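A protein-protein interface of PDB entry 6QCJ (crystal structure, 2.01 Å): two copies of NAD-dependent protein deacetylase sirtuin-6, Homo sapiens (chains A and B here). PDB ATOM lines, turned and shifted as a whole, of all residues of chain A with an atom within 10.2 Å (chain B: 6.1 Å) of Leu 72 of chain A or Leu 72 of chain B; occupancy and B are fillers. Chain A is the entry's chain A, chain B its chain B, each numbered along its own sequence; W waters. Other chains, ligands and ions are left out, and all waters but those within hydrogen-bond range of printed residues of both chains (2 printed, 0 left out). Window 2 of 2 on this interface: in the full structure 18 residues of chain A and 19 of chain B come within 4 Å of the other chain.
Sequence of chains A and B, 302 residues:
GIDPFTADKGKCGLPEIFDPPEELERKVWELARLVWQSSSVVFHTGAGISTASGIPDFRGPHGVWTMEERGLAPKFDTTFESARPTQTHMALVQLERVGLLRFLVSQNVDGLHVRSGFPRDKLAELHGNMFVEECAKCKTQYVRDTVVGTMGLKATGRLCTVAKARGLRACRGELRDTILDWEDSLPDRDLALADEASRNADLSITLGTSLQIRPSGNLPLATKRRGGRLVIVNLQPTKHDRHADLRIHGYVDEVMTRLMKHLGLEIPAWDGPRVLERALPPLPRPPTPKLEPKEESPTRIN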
ATOM      1  N   PHE A  58      17.747 -21.283  16.792  1.00  0.00           N
ATOM      2  CA  PHE A  58      17.158 -21.344  18.134  1.00  0.00           C
ATOM      3  C   PHE A  58      16.479 -20.018  18.516  1.00  0.00           C
ATOM      4  O   PHE A  58      15.381 -20.099  19.206  1.00  0.00           O
ATOM      5  CB  PHE A  58      18.231 -21.841  19.116  1.00  0.00           C
ATOM      6  CG  PHE A  58      18.489 -23.294  18.882  1.00  0.00           C
ATOM      7  CD1 PHE A  58      17.627 -24.243  19.393  1.00  0.00           C
ATOM      8  CD2 PHE A  58      19.505 -23.708  18.026  1.00  0.00           C
ATOM      9  CE1 PHE A  58      17.848 -25.594  19.132  1.00  0.00           C
ATOM     10  CE2 PHE A  58      19.749 -25.053  17.806  1.00  0.00           C
ATOM     11  CZ  PHE A  58      18.886 -25.999  18.324  1.00  0.00           C
ATOM     12  N   PRO A  61      13.887 -14.586  14.955  1.00  0.00           N
ATOM     13  CA  PRO A  61      12.437 -14.380  14.882  1.00  0.00           C
ATOM     14  C   PRO A  61      11.496 -15.584  14.785  1.00  0.00           C
ATOM     15  O   PRO A  61      10.518 -15.592  15.557  1.00  0.00           O
ATOM     16  CB  PRO A  61      12.272 -13.558  13.585  1.00  0.00           C
ATOM     17  CG  PRO A  61      13.563 -12.760  13.488  1.00  0.00           C
ATOM     18  CD  PRO A  61      14.622 -13.461  14.337  1.00  0.00           C
ATOM     19  N   HIS A  62      11.874 -16.569  13.996  1.00  0.00           N
ATOM     20  CA  HIS A  62      11.209 -17.893  13.856  1.00  0.00           C
ATOM     21  C   HIS A  62      12.070 -19.019  14.424  1.00  0.00           C
ATOM     22  O   HIS A  62      11.687 -20.190  14.297  1.00  0.00           O
ATOM     23  CB  HIS A  62      10.715 -18.049  12.417  1.00  0.00           C
ATOM     24  CG  HIS A  62       9.750 -16.979  11.974  1.00  0.00           C
ATOM     25  ND1 HIS A  62       9.007 -17.156  10.785  1.00  0.00           N
ATOM     26  CD2 HIS A  62       9.336 -15.786  12.490  1.00  0.00           C
ATOM     27  CE1 HIS A  62       8.190 -16.144  10.604  1.00  0.00           C
ATOM     28  NE2 HIS A  62       8.373 -15.243  11.626  1.00  0.00           N
ATOM     29  N   GLY A  63      12.971 -18.705  15.364  1.00  0.00           N
ATOM     30  CA  GLY A  63      13.756 -19.738  16.081  1.00  0.00           C
ATOM     31  C   GLY A  63      12.929 -20.743  16.876  1.00  0.00           C
ATOM     32  O   GLY A  63      11.829 -20.362  17.360  1.00  0.00           O
ATOM     33  N   VAL A  64      13.512 -21.909  17.197  1.00  0.00           N
ATOM     34  CA  VAL A  64      12.853 -23.002  18.006  1.00  0.00           C
ATOM     35  C   VAL A  64      12.439 -22.468  19.393  1.00  0.00           C
ATOM     36  O   VAL A  64      11.228 -22.474  19.718  1.00  0.00           O
ATOM     37  CB  VAL A  64      13.728 -24.258  18.134  1.00  0.00           C
ATOM     38  CG1 VAL A  64      12.984 -25.423  18.834  1.00  0.00           C
ATOM     39  CG2 VAL A  64      14.222 -24.750  16.819  1.00  0.00           C
ATOM     40  N   TRP A  65      13.382 -21.926  20.169  1.00  0.00           N
ATOM     41  CA  TRP A  65      13.096 -21.315  21.498  1.00  0.00           C
ATOM     42  C   TRP A  65      12.162 -20.096  21.367  1.00  0.00           C
ATOM     43  O   TRP A  65      11.209 -19.965  22.152  1.00  0.00           O
ATOM     44  CB  TRP A  65      14.389 -20.955  22.232  1.00  0.00           C
ATOM     45  CG  TRP A  65      15.358 -22.084  22.462  1.00  0.00           C
ATOM     46  CD1 TRP A  65      16.670 -21.901  22.808  1.00  0.00           C
ATOM     47  CD2 TRP A  65      15.144 -23.503  22.490  1.00  0.00           C
ATOM     48  NE1 TRP A  65      17.276 -23.092  23.082  1.00  0.00           N
ATOM     49  CE2 TRP A  65      16.377 -24.099  22.851  1.00  0.00           C
ATOM     50  CE3 TRP A  65      14.053 -24.353  22.256  1.00  0.00           C
ATOM     51  CZ2 TRP A  65      16.547 -25.473  22.939  1.00  0.00           C
ATOM     52  CZ3 TRP A  65      14.222 -25.707  22.333  1.00  0.00           C
ATOM     53  CH2 TRP A  65      15.456 -26.263  22.677  1.00  0.00           C
ATOM     54  N   THR A  66      12.370 -19.242  20.385  1.00  0.00           N
ATOM     55  CA  THR A  66      11.481 -18.071  20.177  1.00  0.00           C
ATOM     56  C   THR A  66      10.022 -18.527  19.985  1.00  0.00           C
ATOM     57  O   THR A  66       9.121 -17.904  20.612  1.00  0.00           O
ATOM     58  CB  THR A  66      11.913 -17.245  18.972  1.00  0.00           C
ATOM     59  OG1 THR A  66      13.305 -16.987  19.107  1.00  0.00           O
ATOM     60  CG2 THR A  66      11.089 -15.987  18.819  1.00  0.00           C
ATOM     61  N   MET A  67       9.770 -19.541  19.162  1.00  0.00           N
ATOM     62  CA  MET A  67       8.387 -19.882  18.744  1.00  0.00           C
ATOM     63  C   MET A  67       7.691 -20.540  19.945  1.00  0.00           C
ATOM     64  O   MET A  67       6.682 -20.030  20.423  1.00  0.00           O
ATOM     65  CB  MET A  67       8.398 -20.738  17.463  1.00  0.00           C
ATOM     66  CG  MET A  67       8.806 -19.950  16.207  1.00  0.00           C
ATOM     67  SD  MET A  67       7.809 -18.461  15.764  1.00  0.00           S
ATOM     68  CE  MET A  67       6.837 -19.140  14.419  1.00  0.00           C
ATOM     69  N   GLU A  68       8.312 -21.533  20.556  1.00  0.00           N
ATOM     70  CA  GLU A  68       7.964 -22.038  21.904  1.00  0.00           C
ATOM     71  C   GLU A  68       7.418 -20.914  22.816  1.00  0.00           C
ATOM     72  O   GLU A  68       6.242 -21.050  23.339  1.00  0.00           O
ATOM     73  CB  GLU A  68       9.242 -22.643  22.490  1.00  0.00           C
ATOM     74  CG  GLU A  68       9.013 -23.822  23.375  1.00  0.00           C
ATOM     75  CD  GLU A  68      10.295 -24.518  23.746  1.00  0.00           C
ATOM     76  OE1 GLU A  68      10.928 -24.064  24.725  1.00  0.00           O
ATOM     77  OE2 GLU A  68      10.685 -25.472  23.014  1.00  0.00           O
ATOM     78  N   GLU A  69       8.203 -19.849  23.030  1.00  0.00           N
ATOM     79  CA  GLU A  69       7.885 -18.748  23.984  1.00  0.00           C
ATOM     80  C   GLU A  69       6.585 -18.025  23.613  1.00  0.00           C
ATOM     81  O   GLU A  69       5.848 -17.513  24.564  1.00  0.00           O
ATOM     82  CB  GLU A  69       8.981 -17.717  23.948  1.00  0.00           C
ATOM     83  CG  GLU A  69       9.139 -16.908  25.197  1.00  0.00           C
ATOM     84  CD  GLU A  69      10.396 -16.069  25.027  1.00  0.00           C
ATOM     85  OE1 GLU A  69      10.255 -14.836  24.878  1.00  0.00           O
ATOM     86  OE2 GLU A  69      11.503 -16.673  24.937  1.00  0.00           O
ATOM     87  N   ARG A  70       6.338 -17.875  22.303  1.00  0.00           N
ATOM     88  CA  ARG A  70       5.047 -17.347  21.770  1.00  0.00           C
ATOM     89  C   ARG A  70       4.032 -18.479  21.529  1.00  0.00           C
ATOM     90  O   ARG A  70       2.935 -18.200  20.999  1.00  0.00           O
ATOM     91  CB  ARG A  70       5.262 -16.518  20.515  1.00  0.00           C
ATOM     92  CG  ARG A  70       5.938 -15.176  20.780  1.00  0.00           C
ATOM     93  CD  ARG A  70       7.420 -15.206  20.448  1.00  0.00           C
ATOM     94  NE  ARG A  70       8.190 -13.966  20.609  1.00  0.00           N
ATOM     95  CZ  ARG A  70       9.261 -13.804  21.397  1.00  0.00           C
ATOM     96  NH1 ARG A  70       9.717 -14.799  22.145  1.00  0.00           N
ATOM     97  NH2 ARG A  70       9.869 -12.631  21.433  1.00  0.00           N
ATOM     98  N   GLY A  71       4.343 -19.717  21.900  1.00  0.00           N
ATOM     99  CA  GLY A  71       3.383 -20.843  21.807  1.00  0.00           C
ATOM    100  C   GLY A  71       3.152 -21.352  20.386  1.00  0.00           C
ATOM    101  O   GLY A  71       2.134 -22.056  20.142  1.00  0.00           O
ATOM    102  N   LEU A  72       4.079 -21.109  19.463  1.00  0.00           N
ATOM    103  CA  LEU A  72       3.948 -21.641  18.077  1.00  0.00           C
ATOM    104  C   LEU A  72       5.048 -22.664  17.903  1.00  0.00           C
ATOM    105  O   LEU A  72       5.773 -22.886  18.874  1.00  0.00           O
ATOM    106  CB  LEU A  72       4.040 -20.477  17.087  1.00  0.00           C
ATOM    107  CG  LEU A  72       3.278 -19.237  17.541  1.00  0.00           C
ATOM    108  CD1 LEU A  72       3.567 -18.043  16.664  1.00  0.00           C
ATOM    109  CD2 LEU A  72       1.774 -19.510  17.632  1.00  0.00           C
ATOM    110  N   ALA A  73       5.163 -23.261  16.725  1.00  0.00           N
ATOM    111  CA  ALA A  73       6.165 -24.319  16.463  1.00  0.00           C
ATOM    112  C   ALA A  73       7.164 -23.800  15.429  1.00  0.00           C
ATOM    113  O   ALA A  73       6.849 -22.919  14.611  1.00  0.00           O
ATOM    114  CB  ALA A  73       5.469 -25.637  16.101  1.00  0.00           C
ATOM    115  N   PRO A  74       8.441 -24.246  15.511  1.00  0.00           N
ATOM    116  CA  PRO A  74       9.425 -23.979  14.463  1.00  0.00           C
ATOM    117  C   PRO A  74       8.956 -24.698  13.206  1.00  0.00           C
ATOM    118  O   PRO A  74       8.190 -25.570  13.332  1.00  0.00           O
ATOM    119  CB  PRO A  74      10.723 -24.648  14.903  1.00  0.00           C
ATOM    120  CG  PRO A  74      10.235 -25.660  15.941  1.00  0.00           C
ATOM    121  CD  PRO A  74       9.028 -25.038  16.606  1.00  0.00           C
ATOM    122  N   LYS A  75       9.471 -24.320  12.054  1.00  0.00           N
ATOM    123  CA  LYS A  75       9.107 -25.013  10.787  1.00  0.00           C
ATOM    124  C   LYS A  75      10.373 -25.520  10.086  1.00  0.00           C
ATOM    125  O   LYS A  75      11.306 -24.679   9.870  1.00  0.00           O
ATOM    126  CB  LYS A  75       8.317 -23.942  10.030  1.00  0.00           C
ATOM    127  CG  LYS A  75       7.343 -24.379   8.941  1.00  0.00           C
ATOM    128  CD  LYS A  75       7.432 -25.817   8.504  1.00  0.00           C
ATOM    129  CE  LYS A  75       7.524 -25.908   6.997  1.00  0.00           C
ATOM    130  NZ  LYS A  75       7.516 -27.292   6.507  1.00  0.00           N
ATOM    131  N   HIS B  62       3.995 -21.348   7.821  1.00  0.00           N
ATOM    132  CA  HIS B  62       4.759 -20.050   7.927  1.00  0.00           C
ATOM    133  C   HIS B  62       4.770 -19.304   6.590  1.00  0.00           C
ATOM    134  O   HIS B  62       5.496 -18.341   6.419  1.00  0.00           O
ATOM    135  CB  HIS B  62       6.206 -20.259   8.439  1.00  0.00           C
ATOM    136  CG  HIS B  62       6.242 -20.709   9.868  1.00  0.00           C
ATOM    137  ND1 HIS B  62       7.344 -20.554  10.683  1.00  0.00           N
ATOM    138  CD2 HIS B  62       5.299 -21.303  10.643  1.00  0.00           C
ATOM    139  CE1 HIS B  62       7.083 -21.053  11.877  1.00  0.00           C
ATOM    140  NE2 HIS B  62       5.858 -21.522  11.881  1.00  0.00           N
ATOM    141  N   VAL B  64       3.722 -16.515   3.641  1.00  0.00           N
ATOM    142  CA  VAL B  64       3.484 -15.033   3.647  1.00  0.00           C
ATOM    143  C   VAL B  64       2.019 -14.715   4.017  1.00  0.00           C
ATOM    144  O   VAL B  64       1.767 -14.083   5.105  1.00  0.00           O
ATOM    145  CB  VAL B  64       3.846 -14.398   2.281  1.00  0.00           C
ATOM    146  CG1 VAL B  64       3.530 -12.920   2.258  1.00  0.00           C
ATOM    147  CG2 VAL B  64       5.312 -14.598   1.868  1.00  0.00           C
ATOM    148  N   MET B  67       0.970 -15.826   7.452  1.00  0.00           N
ATOM    149  CA  MET B  67       1.560 -15.074   8.596  1.00  0.00           C
ATOM    150  C   MET B  67       0.893 -13.696   8.724  1.00  0.00           C
ATOM    151  O   MET B  67       0.726 -13.233   9.861  1.00  0.00           O
ATOM    152  CB  MET B  67       3.069 -14.923   8.389  1.00  0.00           C
ATOM    153  CG  MET B  67       3.849 -16.221   8.593  1.00  0.00           C
ATOM    154  SD  MET B  67       3.485 -17.022  10.159  1.00  0.00           S
ATOM    155  CE  MET B  67       5.128 -17.175  10.857  1.00  0.00           C
ATOM    156  N   GLU B  68       0.580 -13.055   7.589  1.00  0.00           N
ATOM    157  CA  GLU B  68      -0.332 -11.885   7.424  1.00  0.00           C
ATOM    158  C   GLU B  68      -1.665 -12.110   8.176  1.00  0.00           C
ATOM    159  O   GLU B  68      -1.955 -11.361   9.118  1.00  0.00           O
ATOM    160  CB  GLU B  68      -0.613 -11.712   5.932  1.00  0.00           C
ATOM    161  CG  GLU B  68      -0.577 -10.290   5.427  1.00  0.00           C
ATOM    162  CD  GLU B  68      -0.406 -10.189   3.919  1.00  0.00           C
ATOM    163  OE1 GLU B  68      -1.353 -10.491   3.175  1.00  0.00           O
ATOM    164  OE2 GLU B  68       0.692  -9.827   3.486  1.00  0.00           O
ATOM    165  N   GLU B  69      -2.463 -13.091   7.744  1.00  0.00           N
ATOM    166  CA  GLU B  69      -3.674 -13.584   8.452  1.00  0.00           C
ATOM    167  C   GLU B  69      -3.435 -13.609   9.972  1.00  0.00           C
ATOM    168  O   GLU B  69      -4.278 -13.058  10.666  1.00  0.00           O
ATOM    169  CB  GLU B  69      -4.018 -14.950   7.886  1.00  0.00           C
ATOM    170  CG  GLU B  69      -5.442 -15.355   8.056  1.00  0.00           C
ATOM    171  CD  GLU B  69      -5.720 -16.638   7.296  1.00  0.00           C
ATOM    172  OE1 GLU B  69      -5.621 -17.725   7.913  1.00  0.00           O
ATOM    173  OE2 GLU B  69      -6.008 -16.547   6.082  1.00  0.00           O
ATOM    174  N   ARG B  70      -2.321 -14.159  10.482  1.00  0.00           N
ATOM    175  CA  ARG B  70      -2.052 -14.209  11.959  1.00  0.00           C
ATOM    176  C   ARG B  70      -1.356 -12.936  12.459  1.00  0.00           C
ATOM    177  O   ARG B  70      -0.949 -12.890  13.650  1.00  0.00           O
ATOM    178  CB  ARG B  70      -1.184 -15.409  12.340  1.00  0.00           C
ATOM    179  N   GLY B  71      -1.190 -11.939  11.592  1.00  0.00           N
ATOM    180  CA  GLY B  71      -0.566 -10.661  11.966  1.00  0.00           C
ATOM    181  C   GLY B  71       0.871 -10.856  12.416  1.00  0.00           C
ATOM    182  O   GLY B  71       1.332 -10.067  13.263  1.00  0.00           O
ATOM    183  N   LEU B  72       1.558 -11.855  11.856  1.00  0.00           N
ATOM    184  CA  LEU B  72       3.026 -12.042  12.009  1.00  0.00           C
ATOM    185  C   LEU B  72       3.691 -11.815  10.644  1.00  0.00           C
ATOM    186  O   LEU B  72       2.966 -11.610   9.645  1.00  0.00           O
ATOM    187  CB  LEU B  72       3.269 -13.436  12.590  1.00  0.00           C
ATOM    188  CG  LEU B  72       2.297 -13.804  13.715  1.00  0.00           C
ATOM    189  CD1 LEU B  72       2.406 -15.272  14.097  1.00  0.00           C
ATOM    190  CD2 LEU B  72       2.514 -12.906  14.926  1.00  0.00           C
ATOM    191  N   ALA B  73       5.021 -11.749  10.600  1.00  0.00           N
ATOM    192  CA  ALA B  73       5.777 -11.432   9.362  1.00  0.00           C
ATOM    193  C   ALA B  73       6.364 -12.712   8.768  1.00  0.00           C
ATOM    194  O   ALA B  73       6.703 -13.646   9.494  1.00  0.00           O
ATOM    195  CB  ALA B  73       6.830 -10.396   9.647  1.00  0.00           C
ATOM    196  N   PRO B  74       6.450 -12.860   7.429  1.00  0.00           N
ATOM    197  CA  PRO B  74       7.270 -13.922   6.827  1.00  0.00           C
ATOM    198  C   PRO B  74       8.738 -13.688   7.140  1.00  0.00           C
ATOM    199  O   PRO B  74       9.118 -12.538   7.284  1.00  0.00           O
ATOM    200  CB  PRO B  74       7.109 -13.777   5.312  1.00  0.00           C
ATOM    201  CG  PRO B  74       6.609 -12.347   5.169  1.00  0.00           C
ATOM    202  CD  PRO B  74       5.765 -12.070   6.400  1.00  0.00           C
HETATM  203  O   HOH W   1      10.344 -21.529  11.971  1.00  0.00           O
HETATM  204  O   HOH W   2       3.755 -22.155  13.985  1.00  0.00           O
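A ring nitrogen (NE2) of His 62 of chain A lies close to the backbone carbonyl oxygen (O) of Ala 73 of chain B (3.1 Å).
A ring nitrogen (NE2) of His 62 of chain B is in hydrogen-bond range of the backbone carbonyl oxygen of Ala 73 of chain A (3.2 Å).
The backbone NH (N) of Leu 72 of chain A lies within hydrogen-bond range of the backbone carbonyl oxygen (O) of Met 67 of chain A (3.0 Å).
N of Leu 72 of chain B sits at hydrogen-bond distance from O of Met 67 of chain B.
His 62 of chain B touches His 62 of chain A (ND1 to ND1, 3.8 Å).
His 62 of chain A touches Met 67 of chain B.
Met 67 of chain A touches His 62 of chain B.
Leu 72 of chain A touches Leu 72 of chain B.
Lys 75 of chain A touches His 62 of chain B.
Of the printed residues of chain B, His 62 of chain A touches His 62 (3.8 Å), Met 67 (3.2 Å) and Ala 73 (3.1 Å).
Leu 72 of chain A touches one residue of chain B.
Printed residues of chain A within 4 Å of His 62 of chain B: His 62 (3.8 Å), Met 67 (3.2 Å), Ala 73 (3.2 Å) and Lys 75 (3.6 Å).
Met 67 of chain B touches one residue of chain A.
Arg 70 of chain B touches none of the printed residues of chain A.
No residue of chain A comes within 4 Å of Gly 71 of chain B.
Leu 72 of chain B touches one residue of chain A.
The nearest printed residue of chain B that does not touch Lys 75 of chain A is Met 67 of chain B (7.5 Å).
Hydrophobic or aromatic side chains of chain B within 4 Å of the printed part of chain A: His 62, Met 67 and Leu 72.
Hydrophobic or aromatic side chains of chain A that line the printed part of chain B: His 62, Met 67 and Leu 72.
Among the printed residues, no Asp or Glu carboxylate lies within 4 Å of a Lys or Arg side-chain nitrogen of the other chain.
His 62 of chain A touches its own counterpart, His 62 of chain B.
His 62 of chain A touches Met 67 of chain B, and with the chains exchanged Met 67 of chain A touches His 62 of chain B.
His 62 of chain A touches Ala 73 of chain B, and with the chains exchanged Ala 73 of chain A touches His 62 of chain B.
Leu 72 of chain B touches its own counterpart, Leu 72 of chain A.
Water W1 lies within hydrogen-bond range of the backbone NH (N) of Lys 75 of chain A (2.9 Å), the backbone carbonyl oxygen (O) of His 62 of chain A (3.0 Å) and a ring nitrogen (ND1) of His 62 of chain B (3.4 Å).
Water W2 lies within hydrogen-bond range of a ring nitrogen (NE2) of His 62 of chain B (3.0 Å) and the backbone carbonyl oxygen (O) of Ala 73 of chain A (3.2 Å).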
